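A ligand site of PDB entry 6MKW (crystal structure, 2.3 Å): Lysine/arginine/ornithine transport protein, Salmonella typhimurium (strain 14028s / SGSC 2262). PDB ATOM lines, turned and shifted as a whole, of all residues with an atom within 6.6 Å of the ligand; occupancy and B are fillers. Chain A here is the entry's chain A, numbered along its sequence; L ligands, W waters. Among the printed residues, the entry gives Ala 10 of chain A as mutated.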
ATOM      1  N   ALA A  10      -4.076 -22.149 -12.436  1.00  0.00           N
ATOM      2  CA  ALA A  10      -4.435 -20.850 -11.869  1.00  0.00           C
ATOM      3  C   ALA A  10      -5.137 -21.136 -10.558  1.00  0.00           C
ATOM      4  O   ALA A  10      -6.313 -21.529 -10.549  1.00  0.00           O
ATOM      5  CB  ALA A  10      -5.322 -20.027 -12.799  1.00  0.00           C
ATOM      6  N   TYR A  13      -9.414 -20.865  -8.259  1.00  0.00           N
ATOM      7  CA  TYR A  13     -10.658 -21.442  -8.765  1.00  0.00           C
ATOM      8  C   TYR A  13     -11.003 -22.644  -7.882  1.00  0.00           C
ATOM      9  O   TYR A  13     -10.963 -23.804  -8.290  1.00  0.00           O
ATOM     10  CB  TYR A  13     -10.534 -21.842 -10.235  1.00  0.00           C
ATOM     11  CG  TYR A  13     -11.676 -21.481 -11.159  1.00  0.00           C
ATOM     12  CD1 TYR A  13     -12.102 -20.160 -11.339  1.00  0.00           C
ATOM     13  CD2 TYR A  13     -12.291 -22.464 -11.936  1.00  0.00           C
ATOM     14  CE1 TYR A  13     -13.134 -19.829 -12.230  1.00  0.00           C
ATOM     15  CE2 TYR A  13     -13.323 -22.147 -12.824  1.00  0.00           C
ATOM     16  CZ  TYR A  13     -13.742 -20.826 -12.973  1.00  0.00           C
ATOM     17  OH  TYR A  13     -14.760 -20.556 -13.846  1.00  0.00           O
ATOM     18  N   PHE A  51      -4.693 -17.304 -15.134  1.00  0.00           N
ATOM     19  CA  PHE A  51      -5.334 -18.202 -16.089  1.00  0.00           C
ATOM     20  C   PHE A  51      -4.977 -17.837 -17.522  1.00  0.00           C
ATOM     21  O   PHE A  51      -4.686 -18.728 -18.334  1.00  0.00           O
ATOM     22  CB  PHE A  51      -6.838 -18.204 -15.919  1.00  0.00           C
ATOM     23  CG  PHE A  51      -7.530 -19.224 -16.786  1.00  0.00           C
ATOM     24  CD1 PHE A  51      -7.497 -20.575 -16.441  1.00  0.00           C
ATOM     25  CD2 PHE A  51      -8.204 -18.848 -17.932  1.00  0.00           C
ATOM     26  CE1 PHE A  51      -8.136 -21.500 -17.208  1.00  0.00           C
ATOM     27  CE2 PHE A  51      -8.849 -19.799 -18.725  1.00  0.00           C
ATOM     28  CZ  PHE A  51      -8.810 -21.123 -18.354  1.00  0.00           C
ATOM     29  N   LEU A  54      -1.741 -19.271 -19.163  1.00  0.00           N
ATOM     30  CA  LEU A  54      -1.486 -20.707 -19.180  1.00  0.00           C
ATOM     31  C   LEU A  54      -1.187 -21.208 -20.587  1.00  0.00           C
ATOM     32  O   LEU A  54      -0.136 -21.822 -20.823  1.00  0.00           O
ATOM     33  CB  LEU A  54      -2.676 -21.456 -18.579  1.00  0.00           C
ATOM     34  CG  LEU A  54      -2.795 -21.341 -17.056  1.00  0.00           C
ATOM     35  CD1 LEU A  54      -4.157 -21.863 -16.572  1.00  0.00           C
ATOM     36  CD2 LEU A  54      -1.659 -22.105 -16.399  1.00  0.00           C
ATOM     37  N   SER A  68      -6.368 -26.912 -15.033  1.00  0.00           N
ATOM     38  CA  SER A  68      -6.860 -25.680 -14.476  1.00  0.00           C
ATOM     39  C   SER A  68      -8.283 -25.424 -14.930  1.00  0.00           C
ATOM     40  O   SER A  68      -8.590 -24.319 -15.380  1.00  0.00           O
ATOM     41  CB  SER A  68      -5.976 -24.517 -14.921  1.00  0.00           C
ATOM     42  OG  SER A  68      -6.101 -23.431 -14.044  1.00  0.00           O
ATOM     43  N   SER A  69      -9.149 -26.435 -14.838  1.00  0.00           N
ATOM     44  CA  SER A  69     -10.536 -26.309 -15.302  1.00  0.00           C
ATOM     45  C   SER A  69     -10.580 -25.831 -16.747  1.00  0.00           C
ATOM     46  O   SER A  69     -11.468 -25.065 -17.116  1.00  0.00           O
ATOM     47  CB  SER A  69     -11.331 -25.351 -14.418  1.00  0.00           C
ATOM     48  OG  SER A  69     -11.560 -25.893 -13.143  1.00  0.00           O
ATOM     49  N   LEU A  70      -9.603 -26.249 -17.550  1.00  0.00           N
ATOM     50  CA  LEU A  70      -9.451 -25.744 -18.916  1.00  0.00           C
ATOM     51  C   LEU A  70     -10.435 -26.472 -19.833  1.00  0.00           C
ATOM     52  O   LEU A  70     -10.269 -27.666 -20.124  1.00  0.00           O
ATOM     53  CB  LEU A  70      -8.025 -25.950 -19.408  1.00  0.00           C
ATOM     54  CG  LEU A  70      -7.693 -25.348 -20.771  1.00  0.00           C
ATOM     55  CD1 LEU A  70      -7.600 -23.837 -20.624  1.00  0.00           C
ATOM     56  CD2 LEU A  70      -6.386 -25.932 -21.310  1.00  0.00           C
ATOM     57  N   SER A  71     -11.466 -25.770 -20.265  1.00  0.00           N
ATOM     58  CA  SER A  71     -12.527 -26.408 -21.040  1.00  0.00           C
ATOM     59  C   SER A  71     -12.053 -26.756 -22.455  1.00  0.00           C
ATOM     60  O   SER A  71     -11.316 -25.995 -23.086  1.00  0.00           O
ATOM     61  CB  SER A  71     -13.740 -25.488 -21.104  1.00  0.00           C
ATOM     62  OG  SER A  71     -14.405 -25.527 -19.869  1.00  0.00           O
ATOM     63  N   ILE A  72     -12.475 -27.915 -22.944  1.00  0.00           N
ATOM     64  CA  ILE A  72     -12.084 -28.415 -24.271  1.00  0.00           C
ATOM     65  C   ILE A  72     -12.995 -27.745 -25.301  1.00  0.00           C
ATOM     66  O   ILE A  72     -14.105 -28.206 -25.525  1.00  0.00           O
ATOM     67  CB  ILE A  72     -12.188 -29.940 -24.341  1.00  0.00           C
ATOM     68  CG1 ILE A  72     -11.472 -30.590 -23.163  1.00  0.00           C
ATOM     69  CG2 ILE A  72     -11.637 -30.474 -25.660  1.00  0.00           C
ATOM     70  CD1 ILE A  72     -11.893 -32.006 -22.875  1.00  0.00           C
ATOM     71  N   THR A  73     -12.540 -26.669 -25.913  1.00  0.00           N
ATOM     72  CA  THR A  73     -13.343 -25.998 -26.929  1.00  0.00           C
ATOM     73  C   THR A  73     -12.745 -26.196 -28.314  1.00  0.00           C
ATOM     74  O   THR A  73     -11.584 -26.586 -28.474  1.00  0.00           O
ATOM     75  CB  THR A  73     -13.450 -24.501 -26.692  1.00  0.00           C
ATOM     76  OG1 THR A  73     -12.169 -23.909 -26.958  1.00  0.00           O
ATOM     77  CG2 THR A  73     -13.941 -24.200 -25.257  1.00  0.00           C
ATOM     78  N   ARG A  76      -9.844 -23.813 -28.942  1.00  0.00           N
ATOM     79  CA  ARG A  76      -8.623 -24.164 -28.230  1.00  0.00           C
ATOM     80  C   ARG A  76      -7.947 -25.352 -28.899  1.00  0.00           C
ATOM     81  O   ARG A  76      -6.723 -25.396 -28.978  1.00  0.00           O
ATOM     82  CB  ARG A  76      -8.917 -24.452 -26.755  1.00  0.00           C
ATOM     83  CG  ARG A  76      -8.881 -23.223 -25.899  1.00  0.00           C
ATOM     84  CD  ARG A  76      -9.444 -23.500 -24.545  1.00  0.00           C
ATOM     85  NE  ARG A  76      -9.604 -22.266 -23.787  1.00  0.00           N
ATOM     86  CZ  ARG A  76     -10.282 -22.169 -22.657  1.00  0.00           C
ATOM     87  NH1 ARG A  76     -10.901 -23.234 -22.161  1.00  0.00           N
ATOM     88  NH2 ARG A  76     -10.360 -20.998 -22.017  1.00  0.00           N
ATOM     89  N   ALA A  89     -18.367 -29.098 -17.132  1.00  0.00           N
ATOM     90  CA  ALA A  89     -18.336 -27.744 -16.610  1.00  0.00           C
ATOM     91  C   ALA A  89     -19.331 -26.864 -17.375  1.00  0.00           C
ATOM     92  O   ALA A  89     -19.051 -26.432 -18.502  1.00  0.00           O
ATOM     93  CB  ALA A  89     -16.928 -27.161 -16.676  1.00  0.00           C
ATOM     94  N   SER A  91     -21.446 -23.157 -17.364  1.00  0.00           N
ATOM     95  CA  SER A  91     -21.337 -21.783 -16.908  1.00  0.00           C
ATOM     96  C   SER A  91     -22.677 -21.301 -16.363  1.00  0.00           C
ATOM     97  O   SER A  91     -23.736 -21.728 -16.825  1.00  0.00           O
ATOM     98  CB  SER A  91     -20.891 -20.836 -18.032  1.00  0.00           C
ATOM     99  OG  SER A  91     -19.638 -21.211 -18.560  1.00  0.00           O
ATOM    100  N   LEU A 116     -13.533 -13.702 -16.019  1.00  0.00           N
ATOM    101  CA  LEU A 116     -12.097 -13.957 -15.947  1.00  0.00           C
ATOM    102  C   LEU A 116     -11.431 -13.817 -17.321  1.00  0.00           C
ATOM    103  O   LEU A 116     -11.856 -14.436 -18.310  1.00  0.00           O
ATOM    104  CB  LEU A 116     -11.850 -15.356 -15.365  1.00  0.00           C
ATOM    105  CG  LEU A 116     -10.387 -15.829 -15.199  1.00  0.00           C
ATOM    106  CD1 LEU A 116      -9.695 -15.106 -14.057  1.00  0.00           C
ATOM    107  CD2 LEU A 116     -10.327 -17.335 -14.978  1.00  0.00           C
ATOM    108  N   GLY A 118      -9.297 -14.486 -20.398  1.00  0.00           N
ATOM    109  CA  GLY A 118      -8.883 -15.714 -21.053  1.00  0.00           C
ATOM    110  C   GLY A 118      -9.886 -16.861 -20.987  1.00  0.00           C
ATOM    111  O   GLY A 118      -9.680 -17.874 -21.670  1.00  0.00           O
ATOM    112  N   SER A 119     -10.951 -16.728 -20.210  1.00  0.00           N
ATOM    113  CA  SER A 119     -11.922 -17.795 -20.053  1.00  0.00           C
ATOM    114  C   SER A 119     -12.915 -17.838 -21.217  1.00  0.00           C
ATOM    115  O   SER A 119     -13.033 -16.906 -22.026  1.00  0.00           O
ATOM    116  CB  SER A 119     -12.682 -17.621 -18.741  1.00  0.00           C
ATOM    117  OG  SER A 119     -13.599 -16.546 -18.827  1.00  0.00           O
ATOM    118  N   THR A 120     -13.649 -18.939 -21.282  1.00  0.00           N
ATOM    119  CA  THR A 120     -14.773 -19.047 -22.207  1.00  0.00           C
ATOM    120  C   THR A 120     -15.888 -18.076 -21.842  1.00  0.00           C
ATOM    121  O   THR A 120     -16.612 -17.597 -22.725  1.00  0.00           O
ATOM    122  CB  THR A 120     -15.293 -20.487 -22.218  1.00  0.00           C
ATOM    123  OG1 THR A 120     -15.722 -20.855 -20.885  1.00  0.00           O
ATOM    124  CG2 THR A 120     -14.193 -21.411 -22.667  1.00  0.00           C
ATOM    125  N   GLN A 121     -16.013 -17.749 -20.548  1.00  0.00           N
ATOM    126  CA  GLN A 121     -17.028 -16.778 -20.140  1.00  0.00           C
ATOM    127  C   GLN A 121     -16.696 -15.393 -20.661  1.00  0.00           C
ATOM    128  O   GLN A 121     -17.599 -14.646 -21.076  1.00  0.00           O
ATOM    129  CB  GLN A 121     -17.181 -16.790 -18.627  1.00  0.00           C
ATOM    130  CG  GLN A 121     -17.840 -18.061 -18.063  1.00  0.00           C
ATOM    131  CD  GLN A 121     -16.820 -19.158 -17.761  1.00  0.00           C
ATOM    132  OE1 GLN A 121     -15.609 -18.913 -17.764  1.00  0.00           O
ATOM    133  NE2 GLN A 121     -17.314 -20.373 -17.495  1.00  0.00           N
ATOM    134  N   GLN A 142     -10.021 -14.953 -10.484  1.00  0.00           N
ATOM    135  CA  GLN A 142     -11.426 -15.077 -10.095  1.00  0.00           C
ATOM    136  C   GLN A 142     -11.677 -14.588  -8.686  1.00  0.00           C
ATOM    137  O   GLN A 142     -12.790 -14.115  -8.386  1.00  0.00           O
ATOM    138  CB  GLN A 142     -11.883 -16.527 -10.237  1.00  0.00           C
ATOM    139  CG  GLN A 142     -13.343 -16.775  -9.837  1.00  0.00           C
ATOM    140  CD  GLN A 142     -14.394 -16.303 -10.877  1.00  0.00           C
ATOM    141  OE1 GLN A 142     -14.131 -16.201 -12.089  1.00  0.00           O
ATOM    142  NE2 GLN A 142     -15.600 -16.056 -10.388  1.00  0.00           N
ATOM    143  N   GLN A 159     -19.008 -17.494 -14.582  1.00  0.00           N
ATOM    144  CA  GLN A 159     -17.883 -18.403 -14.376  1.00  0.00           C
ATOM    145  C   GLN A 159     -18.435 -19.814 -14.343  1.00  0.00           C
ATOM    146  O   GLN A 159     -19.642 -20.008 -14.548  1.00  0.00           O
ATOM    147  CB  GLN A 159     -17.135 -18.065 -13.080  1.00  0.00           C
ATOM    148  CG  GLN A 159     -18.012 -18.140 -11.824  1.00  0.00           C
ATOM    149  CD  GLN A 159     -18.959 -16.958 -11.704  1.00  0.00           C
ATOM    150  OE1 GLN A 159     -18.526 -15.810 -11.616  1.00  0.00           O
ATOM    151  NE2 GLN A 159     -20.252 -17.240 -11.754  1.00  0.00           N
ATOM    152  N   ASP A 160     -17.579 -20.810 -14.132  1.00  0.00           N
ATOM    153  CA  ASP A 160     -18.041 -22.193 -14.094  1.00  0.00           C
ATOM    154  C   ASP A 160     -19.014 -22.369 -12.914  1.00  0.00           C
ATOM    155  O   ASP A 160     -18.833 -21.775 -11.844  1.00  0.00           O
ATOM    156  CB  ASP A 160     -16.880 -23.200 -13.984  1.00  0.00           C
ATOM    157  CG  ASP A 160     -16.136 -23.424 -15.322  1.00  0.00           C
ATOM    158  OD1 ASP A 160     -16.617 -23.004 -16.413  1.00  0.00           O
ATOM    159  OD2 ASP A 160     -15.040 -24.016 -15.288  1.00  0.00           O
ATOM    160  N   PHE A 190     -18.611 -22.892 -24.579  1.00  0.00           N
ATOM    161  CA  PHE A 190     -18.175 -23.397 -23.297  1.00  0.00           C
ATOM    162  C   PHE A 190     -17.493 -24.760 -23.347  1.00  0.00           C
ATOM    163  O   PHE A 190     -16.946 -25.199 -22.329  1.00  0.00           O
ATOM    164  CB  PHE A 190     -19.360 -23.415 -22.347  1.00  0.00           C
ATOM    165  CG  PHE A 190     -19.923 -22.041 -22.096  1.00  0.00           C
ATOM    166  CD1 PHE A 190     -21.243 -21.754 -22.323  1.00  0.00           C
ATOM    167  CD2 PHE A 190     -19.079 -21.013 -21.681  1.00  0.00           C
ATOM    168  CE1 PHE A 190     -21.744 -20.465 -22.117  1.00  0.00           C
ATOM    169  CE2 PHE A 190     -19.548 -19.732 -21.489  1.00  0.00           C
ATOM    170  CZ  PHE A 190     -20.893 -19.458 -21.701  1.00  0.00           C
ATOM    171  N   GLY A 193     -16.666 -30.165 -21.349  1.00  0.00           N
ATOM    172  CA  GLY A 193     -15.925 -30.481 -20.137  1.00  0.00           C
ATOM    173  C   GLY A 193     -14.502 -29.966 -20.216  1.00  0.00           C
ATOM    174  O   GLY A 193     -14.091 -29.286 -21.158  1.00  0.00           O
ATOM    175  N   THR A 194     -13.732 -30.296 -19.185  1.00  0.00           N
ATOM    176  CA  THR A 194     -12.343 -29.853 -19.083  1.00  0.00           C
ATOM    177  C   THR A 194     -11.407 -31.032 -19.324  1.00  0.00           C
ATOM    178  O   THR A 194     -11.793 -32.201 -19.247  1.00  0.00           O
ATOM    179  CB  THR A 194     -12.056 -29.213 -17.712  1.00  0.00           C
ATOM    180  OG1 THR A 194     -11.977 -30.217 -16.684  1.00  0.00           O
ATOM    181  CG2 THR A 194     -13.138 -28.250 -17.360  1.00  0.00           C
HETATM  182  N1  LIG L   1     -13.676 -23.728 -17.870  1.00  0.00           N
HETATM  183  C1  LIG L   1     -13.643 -22.317 -18.330  1.00  0.00           C
HETATM  184  C2  LIG L   1     -12.454 -22.127 -19.289  1.00  0.00           C
HETATM  185  O1  LIG L   1     -11.778 -23.140 -19.566  1.00  0.00           O
HETATM  186  C3  LIG L   1     -13.646 -21.343 -17.123  1.00  0.00           C
HETATM  187  C4  LIG L   1     -12.425 -21.281 -16.269  1.00  0.00           C
HETATM  188  N2  LIG L   1     -11.582 -22.354 -16.078  1.00  0.00           N
HETATM  189  C5  LIG L   1     -11.883 -20.267 -15.565  1.00  0.00           C
HETATM  190  C6  LIG L   1     -10.574 -22.005 -15.289  1.00  0.00           C
HETATM  191  N3  LIG L   1     -10.748 -20.730 -14.956  1.00  0.00           N
HETATM  192  O2  LIG L   1     -12.289 -20.990 -19.773  1.00  0.00           O
HETATM  193  O   HOH W   1     -14.466 -18.375 -15.469  1.00  0.00           O
HETATM  194  O   HOH W   2      -8.800 -19.686 -13.288  1.00  0.00           O
HETATM  195  O   HOH W   3     -16.305 -23.271 -20.215  1.00  0.00           O
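O of Ser 69 sits at hydrogen-bond distance from N1 of the ligand (2.7 Å).
An oxygen (O1) of the ligand lies within hydrogen-bond range of the backbone NH (N) of Ser 71 (2.7 Å).
A nitrogen (N1) of the ligand is in hydrogen-bond range of the side-chain hydroxyl (OG) of Ser 71 (2.8 Å).
The guanidinium group (NH1) of Arg 76 lies within salt-bridge range of an oxygen (O1) of the ligand (2.7 Å).
N of Thr 120 lies within hydrogen-bond range of O2 of the ligand (2.9 Å).
N1 of the ligand is in salt-bridge range of OD2 of Asp 160, 2.9 Å away.
O of Gly 118 is in hydrogen-bond range of NH2 of Arg 76 (3.2 Å).
N of Arg 76 lies within hydrogen-bond range of OG1 of Thr 73 (3.1 Å).
NE2 of Gln 121 lies within hydrogen-bond range of OD1 of Asp 160.
N of Asp 160 sits at hydrogen-bond distance from OH of Tyr 13.
The backbone NH of Ala 10 is in hydrogen-bond range of the side-chain hydroxyl of Ser 68.
The side-chain hydroxyl (OG) of Ser 119 sits close to the backbone NH (N) of Gln 121, at 3.2 Å.
The side-chain amide nitrogen (NE2) of Gln 121 is in hydrogen-bond range of the side-chain hydroxyl (OG) of Ser 91, at 2.7 Å.
The side-chain hydroxyl (OG) of Ser 119 lies within hydrogen-bond range of the backbone carbonyl oxygen (O) of Leu 116, 2.8 Å away.
Residues that only touch the ligand: Tyr 13, Phe 51, Ser 68, Leu 70, Leu 116, Ser 119 and Gln 121.
Hydrophobic or aromatic side chains within 4 Å of the ligand: Tyr 13, Phe 51 and Leu 116.
Within 4 Å of the ligand: Tyr 13, Phe 51, Ser 68, Ser 69, Leu 70, Ser 71, Arg 76, Leu 116, Ser 119, Thr 120, Gln 121 and Asp 160.
The nearest printed residue that does not touch the ligand is Gly 118 (4.5 Å).
Water W1 lies within hydrogen-bond range of OE1 of Gln 121 and OH of Tyr 13.
Water W3 lies within hydrogen-bond range of the side-chain hydroxyl of Thr 120, the backbone carbonyl oxygen of Phe 190 and the side-chain hydroxyl of Ser 71.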
